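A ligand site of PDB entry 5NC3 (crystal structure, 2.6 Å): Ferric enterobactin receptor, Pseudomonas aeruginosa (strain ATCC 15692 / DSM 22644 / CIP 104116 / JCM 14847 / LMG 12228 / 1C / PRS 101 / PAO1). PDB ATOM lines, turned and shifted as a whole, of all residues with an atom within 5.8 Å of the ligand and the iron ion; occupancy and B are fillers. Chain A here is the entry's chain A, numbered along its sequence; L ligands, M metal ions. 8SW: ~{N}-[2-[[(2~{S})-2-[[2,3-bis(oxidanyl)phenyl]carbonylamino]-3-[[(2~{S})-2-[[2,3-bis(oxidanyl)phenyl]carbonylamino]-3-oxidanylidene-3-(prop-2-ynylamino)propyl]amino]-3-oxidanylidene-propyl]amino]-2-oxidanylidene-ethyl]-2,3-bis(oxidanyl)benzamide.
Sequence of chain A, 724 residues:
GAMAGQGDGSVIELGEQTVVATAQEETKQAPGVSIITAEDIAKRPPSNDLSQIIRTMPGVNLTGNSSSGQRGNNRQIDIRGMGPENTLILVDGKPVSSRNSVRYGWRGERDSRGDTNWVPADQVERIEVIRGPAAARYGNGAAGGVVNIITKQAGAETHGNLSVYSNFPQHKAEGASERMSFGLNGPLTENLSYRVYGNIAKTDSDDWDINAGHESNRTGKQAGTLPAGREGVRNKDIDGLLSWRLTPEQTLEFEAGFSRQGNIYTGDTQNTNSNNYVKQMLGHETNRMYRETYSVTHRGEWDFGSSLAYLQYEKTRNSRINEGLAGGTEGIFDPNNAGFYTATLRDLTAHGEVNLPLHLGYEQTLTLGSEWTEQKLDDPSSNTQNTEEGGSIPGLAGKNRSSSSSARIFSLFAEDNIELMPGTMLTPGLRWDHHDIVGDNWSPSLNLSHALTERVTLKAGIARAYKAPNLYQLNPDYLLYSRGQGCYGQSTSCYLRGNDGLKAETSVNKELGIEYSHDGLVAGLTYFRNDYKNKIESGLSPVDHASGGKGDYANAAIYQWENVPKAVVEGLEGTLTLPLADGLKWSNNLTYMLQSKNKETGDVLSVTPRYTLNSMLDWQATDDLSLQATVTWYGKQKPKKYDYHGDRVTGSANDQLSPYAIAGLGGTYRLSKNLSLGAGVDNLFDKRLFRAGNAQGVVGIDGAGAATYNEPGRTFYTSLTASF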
ATOM      1  N   ARG A 107      19.395 -12.757   2.956  1.00  0.00           N
ATOM      2  CA  ARG A 107      19.509 -14.168   3.351  1.00  0.00           C
ATOM      3  C   ARG A 107      19.231 -14.387   4.816  1.00  0.00           C
ATOM      4  O   ARG A 107      19.338 -15.501   5.262  1.00  0.00           O
ATOM      5  CB  ARG A 107      20.903 -14.694   3.009  1.00  0.00           C
ATOM      6  CG  ARG A 107      21.385 -14.359   1.605  1.00  0.00           C
ATOM      7  CD  ARG A 107      20.474 -14.987   0.553  1.00  0.00           C
ATOM      8  NE  ARG A 107      20.567 -14.339  -0.760  1.00  0.00           N
ATOM      9  CZ  ARG A 107      19.861 -14.714  -1.831  1.00  0.00           C
ATOM     10  NH1 ARG A 107      19.029 -15.745  -1.733  1.00  0.00           N
ATOM     11  NH2 ARG A 107      19.987 -14.079  -3.003  1.00  0.00           N
ATOM     12  N   LYS A 221      38.933 -12.193 -11.109  1.00  0.00           N
ATOM     13  CA  LYS A 221      39.276 -11.015 -10.331  1.00  0.00           C
ATOM     14  C   LYS A 221      39.152 -11.313  -8.843  1.00  0.00           C
ATOM     15  O   LYS A 221      39.681 -10.587  -8.037  1.00  0.00           O
ATOM     16  CB  LYS A 221      38.355  -9.846 -10.698  1.00  0.00           C
ATOM     17  CG  LYS A 221      38.556  -9.356 -12.117  1.00  0.00           C
ATOM     18  CD  LYS A 221      37.488  -8.358 -12.535  1.00  0.00           C
ATOM     19  CE  LYS A 221      37.616  -7.971 -13.996  1.00  0.00           C
ATOM     20  NZ  LYS A 221      36.524  -7.061 -14.423  1.00  0.00           N
ATOM     21  N   GLN A 222      38.465 -12.399  -8.510  1.00  0.00           N
ATOM     22  CA  GLN A 222      38.320 -12.799  -7.111  1.00  0.00           C
ATOM     23  C   GLN A 222      39.515 -13.591  -6.600  1.00  0.00           C
ATOM     24  O   GLN A 222      39.574 -13.936  -5.407  1.00  0.00           O
ATOM     25  CB  GLN A 222      37.032 -13.615  -6.902  1.00  0.00           C
ATOM     26  CG  GLN A 222      35.750 -12.951  -7.397  1.00  0.00           C
ATOM     27  CD  GLN A 222      35.547 -11.546  -6.863  1.00  0.00           C
ATOM     28  OE1 GLN A 222      36.137 -11.150  -5.847  1.00  0.00           O
ATOM     29  NE2 GLN A 222      34.669 -10.799  -7.521  1.00  0.00           N
ATOM     30  N   ASN A 271      29.915 -11.396   0.896  1.00  0.00           N
ATOM     31  CA  ASN A 271      30.156 -12.394  -0.128  1.00  0.00           C
ATOM     32  C   ASN A 271      31.575 -12.930  -0.209  1.00  0.00           C
ATOM     33  O   ASN A 271      31.828 -13.818  -0.983  1.00  0.00           O
ATOM     34  CB  ASN A 271      29.694 -11.865  -1.491  1.00  0.00           C
ATOM     35  CG  ASN A 271      28.278 -11.296  -1.449  1.00  0.00           C
ATOM     36  OD1 ASN A 271      27.293 -12.010  -1.185  1.00  0.00           O
ATOM     37  ND2 ASN A 271      28.170  -9.996  -1.701  1.00  0.00           N
ATOM     38  N   ASN A 273      34.092 -11.478  -1.407  1.00  0.00           N
ATOM     39  CA  ASN A 273      34.799 -10.627  -2.359  1.00  0.00           C
ATOM     40  C   ASN A 273      35.512  -9.515  -1.604  1.00  0.00           C
ATOM     41  O   ASN A 273      35.241  -9.300  -0.429  1.00  0.00           O
ATOM     42  CB  ASN A 273      33.822  -9.991  -3.341  1.00  0.00           C
ATOM     43  CG  ASN A 273      32.604  -9.393  -2.632  1.00  0.00           C
ATOM     44  OD1 ASN A 273      32.264  -9.782  -1.515  1.00  0.00           O
ATOM     45  ND2 ASN A 273      31.956  -8.456  -3.293  1.00  0.00           N
ATOM     46  N   ALA A 326      23.520  -4.049  -3.312  1.00  0.00           N
ATOM     47  CA  ALA A 326      23.186  -4.626  -4.609  1.00  0.00           C
ATOM     48  C   ALA A 326      24.105  -5.780  -4.963  1.00  0.00           C
ATOM     49  O   ALA A 326      25.315  -5.617  -5.124  1.00  0.00           O
ATOM     50  CB  ALA A 326      23.309  -3.538  -5.657  1.00  0.00           C
ATOM     51  N   GLY A 327      23.490  -6.959  -5.165  1.00  0.00           N
ATOM     52  CA  GLY A 327      24.192  -8.144  -5.614  1.00  0.00           C
ATOM     53  C   GLY A 327      25.491  -8.446  -4.870  1.00  0.00           C
ATOM     54  O   GLY A 327      25.509  -8.601  -3.646  1.00  0.00           O
ATOM     55  N   GLY A 328      26.598  -8.526  -5.598  1.00  0.00           N
ATOM     56  CA  GLY A 328      27.872  -8.629  -4.951  1.00  0.00           C
ATOM     57  C   GLY A 328      28.230  -7.449  -4.061  1.00  0.00           C
ATOM     58  O   GLY A 328      28.993  -7.611  -3.096  1.00  0.00           O
ATOM     59  N   THR A 329      27.716  -6.258  -4.334  1.00  0.00           N
ATOM     60  CA  THR A 329      28.093  -5.118  -3.465  1.00  0.00           C
ATOM     61  C   THR A 329      27.380  -5.145  -2.121  1.00  0.00           C
ATOM     62  O   THR A 329      27.614  -4.266  -1.290  1.00  0.00           O
ATOM     63  CB  THR A 329      27.922  -3.705  -4.104  1.00  0.00           C
ATOM     64  OG1 THR A 329      26.562  -3.484  -4.536  1.00  0.00           O
ATOM     65  CG2 THR A 329      28.897  -3.494  -5.269  1.00  0.00           C
ATOM     66  N   GLU A 330      26.422  -6.042  -1.980  1.00  0.00           N
ATOM     67  CA  GLU A 330      25.696  -6.202  -0.727  1.00  0.00           C
ATOM     68  C   GLU A 330      26.681  -6.604   0.343  1.00  0.00           C
ATOM     69  O   GLU A 330      27.376  -7.612   0.208  1.00  0.00           O
ATOM     70  CB  GLU A 330      24.562  -7.253  -0.828  1.00  0.00           C
ATOM     71  CG  GLU A 330      23.551  -7.220   0.323  1.00  0.00           C
ATOM     72  CD  GLU A 330      22.620  -8.443   0.381  1.00  0.00           C
ATOM     73  OE1 GLU A 330      22.664  -9.277  -0.561  1.00  0.00           O
ATOM     74  OE2 GLU A 330      21.848  -8.582   1.382  1.00  0.00           O
ATOM     75  N   GLU A 389      18.880   1.405 -12.542  1.00  0.00           N
ATOM     76  CA  GLU A 389      19.285   0.303 -13.373  1.00  0.00           C
ATOM     77  C   GLU A 389      18.140  -0.687 -13.591  1.00  0.00           C
ATOM     78  O   GLU A 389      17.932  -1.175 -14.703  1.00  0.00           O
ATOM     79  CB  GLU A 389      20.498  -0.426 -12.766  1.00  0.00           C
ATOM     80  CG  GLU A 389      21.058  -1.519 -13.669  1.00  0.00           C
ATOM     81  CD  GLU A 389      22.455  -2.011 -13.275  1.00  0.00           C
ATOM     82  OE1 GLU A 389      23.444  -1.310 -13.630  1.00  0.00           O
ATOM     83  OE2 GLU A 389      22.565  -3.098 -12.656  1.00  0.00           O
ATOM     84  N   TYR A 481      18.828  -5.288  -4.410  1.00  0.00           N
ATOM     85  CA  TYR A 481      18.843  -5.460  -5.848  1.00  0.00           C
ATOM     86  C   TYR A 481      19.912  -6.487  -6.245  1.00  0.00           C
ATOM     87  O   TYR A 481      20.952  -6.650  -5.586  1.00  0.00           O
ATOM     88  CB  TYR A 481      19.072  -4.077  -6.497  1.00  0.00           C
ATOM     89  CG  TYR A 481      19.388  -4.091  -7.966  1.00  0.00           C
ATOM     90  CD1 TYR A 481      18.412  -4.341  -8.923  1.00  0.00           C
ATOM     91  CD2 TYR A 481      20.671  -3.800  -8.405  1.00  0.00           C
ATOM     92  CE1 TYR A 481      18.733  -4.354 -10.272  1.00  0.00           C
ATOM     93  CE2 TYR A 481      21.001  -3.794  -9.742  1.00  0.00           C
ATOM     94  CZ  TYR A 481      20.032  -4.077 -10.671  1.00  0.00           C
ATOM     95  OH  TYR A 481      20.382  -4.084 -11.997  1.00  0.00           O
ATOM     96  N   SER A 482      19.604  -7.246  -7.282  1.00  0.00           N
ATOM     97  CA  SER A 482      20.603  -8.103  -7.892  1.00  0.00           C
ATOM     98  C   SER A 482      20.356  -8.160  -9.356  1.00  0.00           C
ATOM     99  O   SER A 482      19.210  -8.079  -9.796  1.00  0.00           O
ATOM    100  CB  SER A 482      20.607  -9.532  -7.324  1.00  0.00           C
ATOM    101  OG  SER A 482      21.345 -10.429  -8.162  1.00  0.00           O
ATOM    102  N   ARG A 483      21.429  -8.326 -10.111  1.00  0.00           N
ATOM    103  CA  ARG A 483      21.338  -8.433 -11.550  1.00  0.00           C
ATOM    104  C   ARG A 483      20.967  -9.834 -12.026  1.00  0.00           C
ATOM    105  O   ARG A 483      20.956 -10.073 -13.229  1.00  0.00           O
ATOM    106  CB  ARG A 483      22.683  -8.062 -12.160  1.00  0.00           C
ATOM    107  CG  ARG A 483      23.090  -6.613 -11.931  1.00  0.00           C
ATOM    108  CD  ARG A 483      24.519  -6.389 -12.376  1.00  0.00           C
ATOM    109  NE  ARG A 483      24.824  -4.977 -12.526  1.00  0.00           N
ATOM    110  CZ  ARG A 483      25.969  -4.399 -12.168  1.00  0.00           C
ATOM    111  NH1 ARG A 483      26.965  -5.122 -11.633  1.00  0.00           N
ATOM    112  NH2 ARG A 483      26.119  -3.087 -12.345  1.00  0.00           N
ATOM    113  N   GLY A 484      20.778 -10.769 -11.101  1.00  0.00           N
ATOM    114  CA  GLY A 484      20.404 -12.118 -11.472  1.00  0.00           C
ATOM    115  C   GLY A 484      20.951 -13.225 -10.609  1.00  0.00           C
ATOM    116  O   GLY A 484      20.304 -14.262 -10.420  1.00  0.00           O
ATOM    117  N   GLN A 485      22.137 -13.015 -10.055  1.00  0.00           N
ATOM    118  CA  GLN A 485      22.804 -14.096  -9.343  1.00  0.00           C
ATOM    119  C   GLN A 485      22.123 -14.465  -8.023  1.00  0.00           C
ATOM    120  O   GLN A 485      22.159 -15.624  -7.594  1.00  0.00           O
ATOM    121  CB  GLN A 485      24.276 -13.762  -9.156  1.00  0.00           C
ATOM    122  CG  GLN A 485      25.126 -14.957  -8.794  1.00  0.00           C
ATOM    123  CD  GLN A 485      26.588 -14.799  -9.183  1.00  0.00           C
ATOM    124  OE1 GLN A 485      27.348 -15.762  -9.170  1.00  0.00           O
ATOM    125  NE2 GLN A 485      26.983 -13.577  -9.532  1.00  0.00           N
ATOM    126  N   GLY A 486      21.422 -13.492  -7.418  1.00  0.00           N
ATOM    127  CA  GLY A 486      20.614 -13.753  -6.228  1.00  0.00           C
ATOM    128  C   GLY A 486      19.118 -14.003  -6.461  1.00  0.00           C
ATOM    129  O   GLY A 486      18.390 -14.329  -5.531  1.00  0.00           O
ATOM    130  N   SER A 491      17.874 -15.801 -14.054  1.00  0.00           N
ATOM    131  CA  SER A 491      19.080 -14.971 -14.016  1.00  0.00           C
ATOM    132  C   SER A 491      18.855 -13.509 -14.343  1.00  0.00           C
ATOM    133  O   SER A 491      19.820 -12.759 -14.394  1.00  0.00           O
ATOM    134  CB  SER A 491      20.131 -15.543 -14.963  1.00  0.00           C
ATOM    135  OG  SER A 491      20.702 -16.708 -14.414  1.00  0.00           O
ATOM    136  N   TYR A 553      19.232  -5.255 -17.872  1.00  0.00           N
ATOM    137  CA  TYR A 553      18.731  -5.205 -16.491  1.00  0.00           C
ATOM    138  C   TYR A 553      17.391  -4.436 -16.349  1.00  0.00           C
ATOM    139  O   TYR A 553      16.807  -4.341 -15.240  1.00  0.00           O
ATOM    140  CB  TYR A 553      19.790  -4.584 -15.582  1.00  0.00           C
ATOM    141  CG  TYR A 553      21.195  -5.130 -15.784  1.00  0.00           C
ATOM    142  CD1 TYR A 553      21.491  -6.470 -15.525  1.00  0.00           C
ATOM    143  CD2 TYR A 553      22.224  -4.306 -16.208  1.00  0.00           C
ATOM    144  CE1 TYR A 553      22.777  -6.963 -15.700  1.00  0.00           C
ATOM    145  CE2 TYR A 553      23.511  -4.778 -16.382  1.00  0.00           C
ATOM    146  CZ  TYR A 553      23.778  -6.106 -16.133  1.00  0.00           C
ATOM    147  OH  TYR A 553      25.068  -6.556 -16.335  1.00  0.00           O
ATOM    148  N   TYR A 644      20.592 -19.624  -4.551  1.00  0.00           N
ATOM    149  CA  TYR A 644      19.707 -18.481  -4.477  1.00  0.00           C
ATOM    150  C   TYR A 644      18.675 -18.587  -5.577  1.00  0.00           C
ATOM    151  O   TYR A 644      17.527 -18.150  -5.419  1.00  0.00           O
ATOM    152  CB  TYR A 644      20.486 -17.192  -4.640  1.00  0.00           C
ATOM    153  CG  TYR A 644      21.626 -17.062  -3.662  1.00  0.00           C
ATOM    154  CD1 TYR A 644      21.493 -17.517  -2.357  1.00  0.00           C
ATOM    155  CD2 TYR A 644      22.819 -16.471  -4.024  1.00  0.00           C
ATOM    156  CE1 TYR A 644      22.525 -17.396  -1.457  1.00  0.00           C
ATOM    157  CE2 TYR A 644      23.862 -16.341  -3.122  1.00  0.00           C
ATOM    158  CZ  TYR A 644      23.720 -16.813  -1.839  1.00  0.00           C
ATOM    159  OH  TYR A 644      24.763 -16.682  -0.947  1.00  0.00           O
ATOM    160  N   VAL A 698      29.416 -18.347  -6.111  1.00  0.00           N
ATOM    161  CA  VAL A 698      29.122 -17.220  -7.009  1.00  0.00           C
ATOM    162  C   VAL A 698      30.246 -17.096  -8.041  1.00  0.00           C
ATOM    163  O   VAL A 698      31.215 -17.853  -7.972  1.00  0.00           O
ATOM    164  CB  VAL A 698      28.963 -15.895  -6.237  1.00  0.00           C
ATOM    165  CG1 VAL A 698      27.589 -15.817  -5.576  1.00  0.00           C
ATOM    166  CG2 VAL A 698      30.038 -15.739  -5.161  1.00  0.00           C
ATOM    167  N   VAL A 699      30.105 -16.173  -8.996  1.00  0.00           N
ATOM    168  CA  VAL A 699      31.073 -15.988 -10.072  1.00  0.00           C
ATOM    169  C   VAL A 699      32.488 -15.828  -9.539  1.00  0.00           C
ATOM    170  O   VAL A 699      32.735 -14.938  -8.737  1.00  0.00           O
ATOM    171  CB  VAL A 699      30.733 -14.743 -10.914  1.00  0.00           C
ATOM    172  CG1 VAL A 699      31.874 -14.415 -11.870  1.00  0.00           C
ATOM    173  CG2 VAL A 699      29.460 -14.950 -11.704  1.00  0.00           C
ATOM    174  N   ILE A 701      33.973 -17.462  -7.397  1.00  0.00           N
ATOM    175  CA  ILE A 701      34.091 -17.807  -5.969  1.00  0.00           C
ATOM    176  C   ILE A 701      33.385 -19.127  -5.714  1.00  0.00           C
ATOM    177  O   ILE A 701      32.190 -19.190  -5.555  1.00  0.00           O
ATOM    178  CB  ILE A 701      33.528 -16.736  -5.038  1.00  0.00           C
ATOM    179  CG1 ILE A 701      34.196 -15.383  -5.303  1.00  0.00           C
ATOM    180  CG2 ILE A 701      33.710 -17.157  -3.583  1.00  0.00           C
ATOM    181  CD1 ILE A 701      33.916 -14.336  -4.238  1.00  0.00           C
HETATM  182  OAM 8SW L   1      26.625 -10.037 -10.558  1.00  0.00           O
HETATM  183  CBS 8SW L   1      25.941 -10.670 -11.556  1.00  0.00           C
HETATM  184  CBP 8SW L   1      24.643 -11.076 -11.308  1.00  0.00           C
HETATM  185  OAJ 8SW L   1      24.159 -10.836 -10.052  1.00  0.00           O
HETATM  186  CAT 8SW L   1      23.930 -11.716 -12.329  1.00  0.00           C
HETATM  187  CAQ 8SW L   1      24.525 -11.931 -13.577  1.00  0.00           C
HETATM  188  CAW 8SW L   1      25.833 -11.507 -13.803  1.00  0.00           C
HETATM  189  CBV 8SW L   1      26.539 -10.835 -12.800  1.00  0.00           C
HETATM  190  CBK 8SW L   1      27.853 -10.473 -13.011  1.00  0.00           C
HETATM  191  OAE 8SW L   1      28.557 -11.252 -13.652  1.00  0.00           O
HETATM  192  NBG 8SW L   1      28.375  -9.426 -12.333  1.00  0.00           N
HETATM  193  CBX 8SW L   1      29.836  -9.182 -12.403  1.00  0.00           C
HETATM  194  CBL 8SW L   1      30.555 -10.221 -11.495  1.00  0.00           C
HETATM  195  OAF 8SW L   1      30.040 -11.302 -11.202  1.00  0.00           O
HETATM  196  NBB 8SW L   1      31.787  -9.879 -11.120  1.00  0.00           N
HETATM  197  CAX 8SW L   1      32.683 -10.728 -10.318  1.00  0.00           C
HETATM  198  CAN 8SW L   1      33.986  -9.998 -10.332  1.00  0.00           C
HETATM  199  CAA 8SW L   1      35.035  -9.388 -10.198  1.00  0.00           C
HETATM  200  CBA 8SW L   1      30.255  -7.735 -12.032  1.00  0.00           C
HETATM  201  NBE 8SW L   1      30.047  -7.422 -10.605  1.00  0.00           N
HETATM  202  C   8SW L   1      31.022  -7.402  -9.655  1.00  0.00           C
HETATM  203  O   8SW L   1      32.199  -7.715  -9.873  1.00  0.00           O
HETATM  204  CA  8SW L   1      30.558  -6.996  -8.235  1.00  0.00           C
HETATM  205  N   8SW L   1      29.081  -6.862  -8.228  1.00  0.00           N
HETATM  206  CBJ 8SW L   1      28.509  -5.694  -8.566  1.00  0.00           C
HETATM  207  OAD 8SW L   1      29.180  -4.710  -8.868  1.00  0.00           O
HETATM  208  CBU 8SW L   1      27.103  -5.637  -8.651  1.00  0.00           C
HETATM  209  CAV 8SW L   1      26.489  -4.381  -8.663  1.00  0.00           C
HETATM  210  CAP 8SW L   1      25.098  -4.262  -8.783  1.00  0.00           C
HETATM  211  CAS 8SW L   1      24.311  -5.398  -8.911  1.00  0.00           C
HETATM  212  CBO 8SW L   1      24.906  -6.653  -8.909  1.00  0.00           C
HETATM  213  OAI 8SW L   1      24.219  -7.814  -9.043  1.00  0.00           O
HETATM  214  CBR 8SW L   1      26.278  -6.760  -8.800  1.00  0.00           C
HETATM  215  OAL 8SW L   1      26.793  -8.019  -8.813  1.00  0.00           O
HETATM  216  CB  8SW L   1      31.030  -8.032  -7.200  1.00  0.00           C
HETATM  217  NBD 8SW L   1      30.531  -9.400  -7.500  1.00  0.00           N
HETATM  218  CBH 8SW L   1      31.000 -10.432  -6.786  1.00  0.00           C
HETATM  219  OAB 8SW L   1      31.855 -10.279  -5.923  1.00  0.00           O
HETATM  220  CAY 8SW L   1      30.429 -11.835  -7.102  1.00  0.00           C
HETATM  221  NBC 8SW L   1      28.957 -11.834  -6.943  1.00  0.00           N
HETATM  222  CBI 8SW L   1      28.317 -12.191  -5.800  1.00  0.00           C
HETATM  223  OAC 8SW L   1      28.937 -12.559  -4.799  1.00  0.00           O
HETATM  224  CBT 8SW L   1      26.903 -12.143  -5.766  1.00  0.00           C
HETATM  225  CAU 8SW L   1      26.233 -12.764  -4.694  1.00  0.00           C
HETATM  226  CAO 8SW L   1      24.833 -12.753  -4.581  1.00  0.00           C
HETATM  227  CAR 8SW L   1      24.045 -12.129  -5.544  1.00  0.00           C
HETATM  228  CBN 8SW L   1      24.686 -11.506  -6.617  1.00  0.00           C
HETATM  229  OAH 8SW L   1      24.021 -10.864  -7.631  1.00  0.00           O
HETATM  230  CBQ 8SW L   1      26.074 -11.527  -6.721  1.00  0.00           C
HETATM  231  OAK 8SW L   1      26.616 -10.889  -7.799  1.00  0.00           O
HETATM  232 FE    FE M   1      25.240  -9.470  -8.796  1.00  0.00          FE
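Lys 221 touches the ligand.
Asn 271 touches the ligand.
CB of Ala 326 touches CAP of the ligand, 3.7 Å away.
CA of Gly 327 touches OAH of the ligand, at 3.4 Å.
CG2 of Thr 329 touches OAD of the ligand (3.8 Å).
Tyr 481 touches the ligand (CE2 to CAS, 3.8 Å).
Gly 484 touches the ligand.
Gly 486 touches the ligand.
Tyr 644 touches the ligand (CE2 to CAO, 3.99 Å).
Val 698 touches the ligand.
CB of Val 699 touches OAF of the ligand, at 3.5 Å.
Along chain A the residues within 4 Å of the ligand span positions 221 to 699.
The nearest printed residue that does not touch the ligand is Ser 491 (4.7 Å).
Residues that only touch the iron ion: Gly 327 (3.6 Å) and Gly 328 (3.6 Å).
Of the 23 residues printed, 2 come within 4 Å of the iron ion.
OH of Tyr 481 is in hydrogen-bond range of OE2 of Glu 389 (2.5 Å).
The side-chain hydroxyl (OG1) of Thr 329 is in hydrogen-bond range of the backbone carbonyl oxygen (O) of Ala 326, at 2.5 Å.
The backbone NH of Gln 485 is in hydrogen-bond range of the side-chain hydroxyl of Ser 482, 3.3 Å away.
The guanidinium group (NH2) of Arg 107 sits at hydrogen-bond distance from the backbone carbonyl oxygen (O) of Gly 486, 3.0 Å away.
The backbone carbonyl oxygen of Gly 328 sits at hydrogen-bond distance from the side-chain amide nitrogen of Asn 273 (3.1 Å).
The backbone NH (N) of Gly 486 lies within hydrogen-bond range of the side-chain hydroxyl (OG) of Ser 482, at 3.2 Å.
The backbone carbonyl oxygen (O) of Tyr 481 is in hydrogen-bond range of the backbone NH (N) of Gly 327, 2.6 Å away.
NE of Arg 483 lies within salt-bridge range of OE2 of Glu 389 (2.9 Å).
The iron ion is bound by OAI of the ligand (2.0 Å), OAL of the ligand (2.1 Å), OAJ of the ligand (2.1 Å), OAH of the ligand (2.2 Å), OAK of the ligand (2.2 Å) and OAM of the ligand (2.3 Å).
An oxygen (OAJ) of the ligand lies close to the backbone NH (N) of Gln 485.
The backbone NH (N) of Gly 328 sits close to an oxygen (OAK) of the ligand, 3.2 Å away.
NE2 of Gln 485 sits close to OAK of the ligand.
The side-chain hydroxyl (OG) of Ser 482 lies close to an oxygen (OAH) of the ligand, at 2.8 Å.
The side-chain amide nitrogen (ND2) of Asn 273 is in hydrogen-bond range of an oxygen (OAB) of the ligand, at 3.2 Å.
NE2 of Gln 222 sits close to OAB of the ligand (3.3 Å).
The backbone NH of Arg 483 lies close to an oxygen (OAI) of the ligand.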
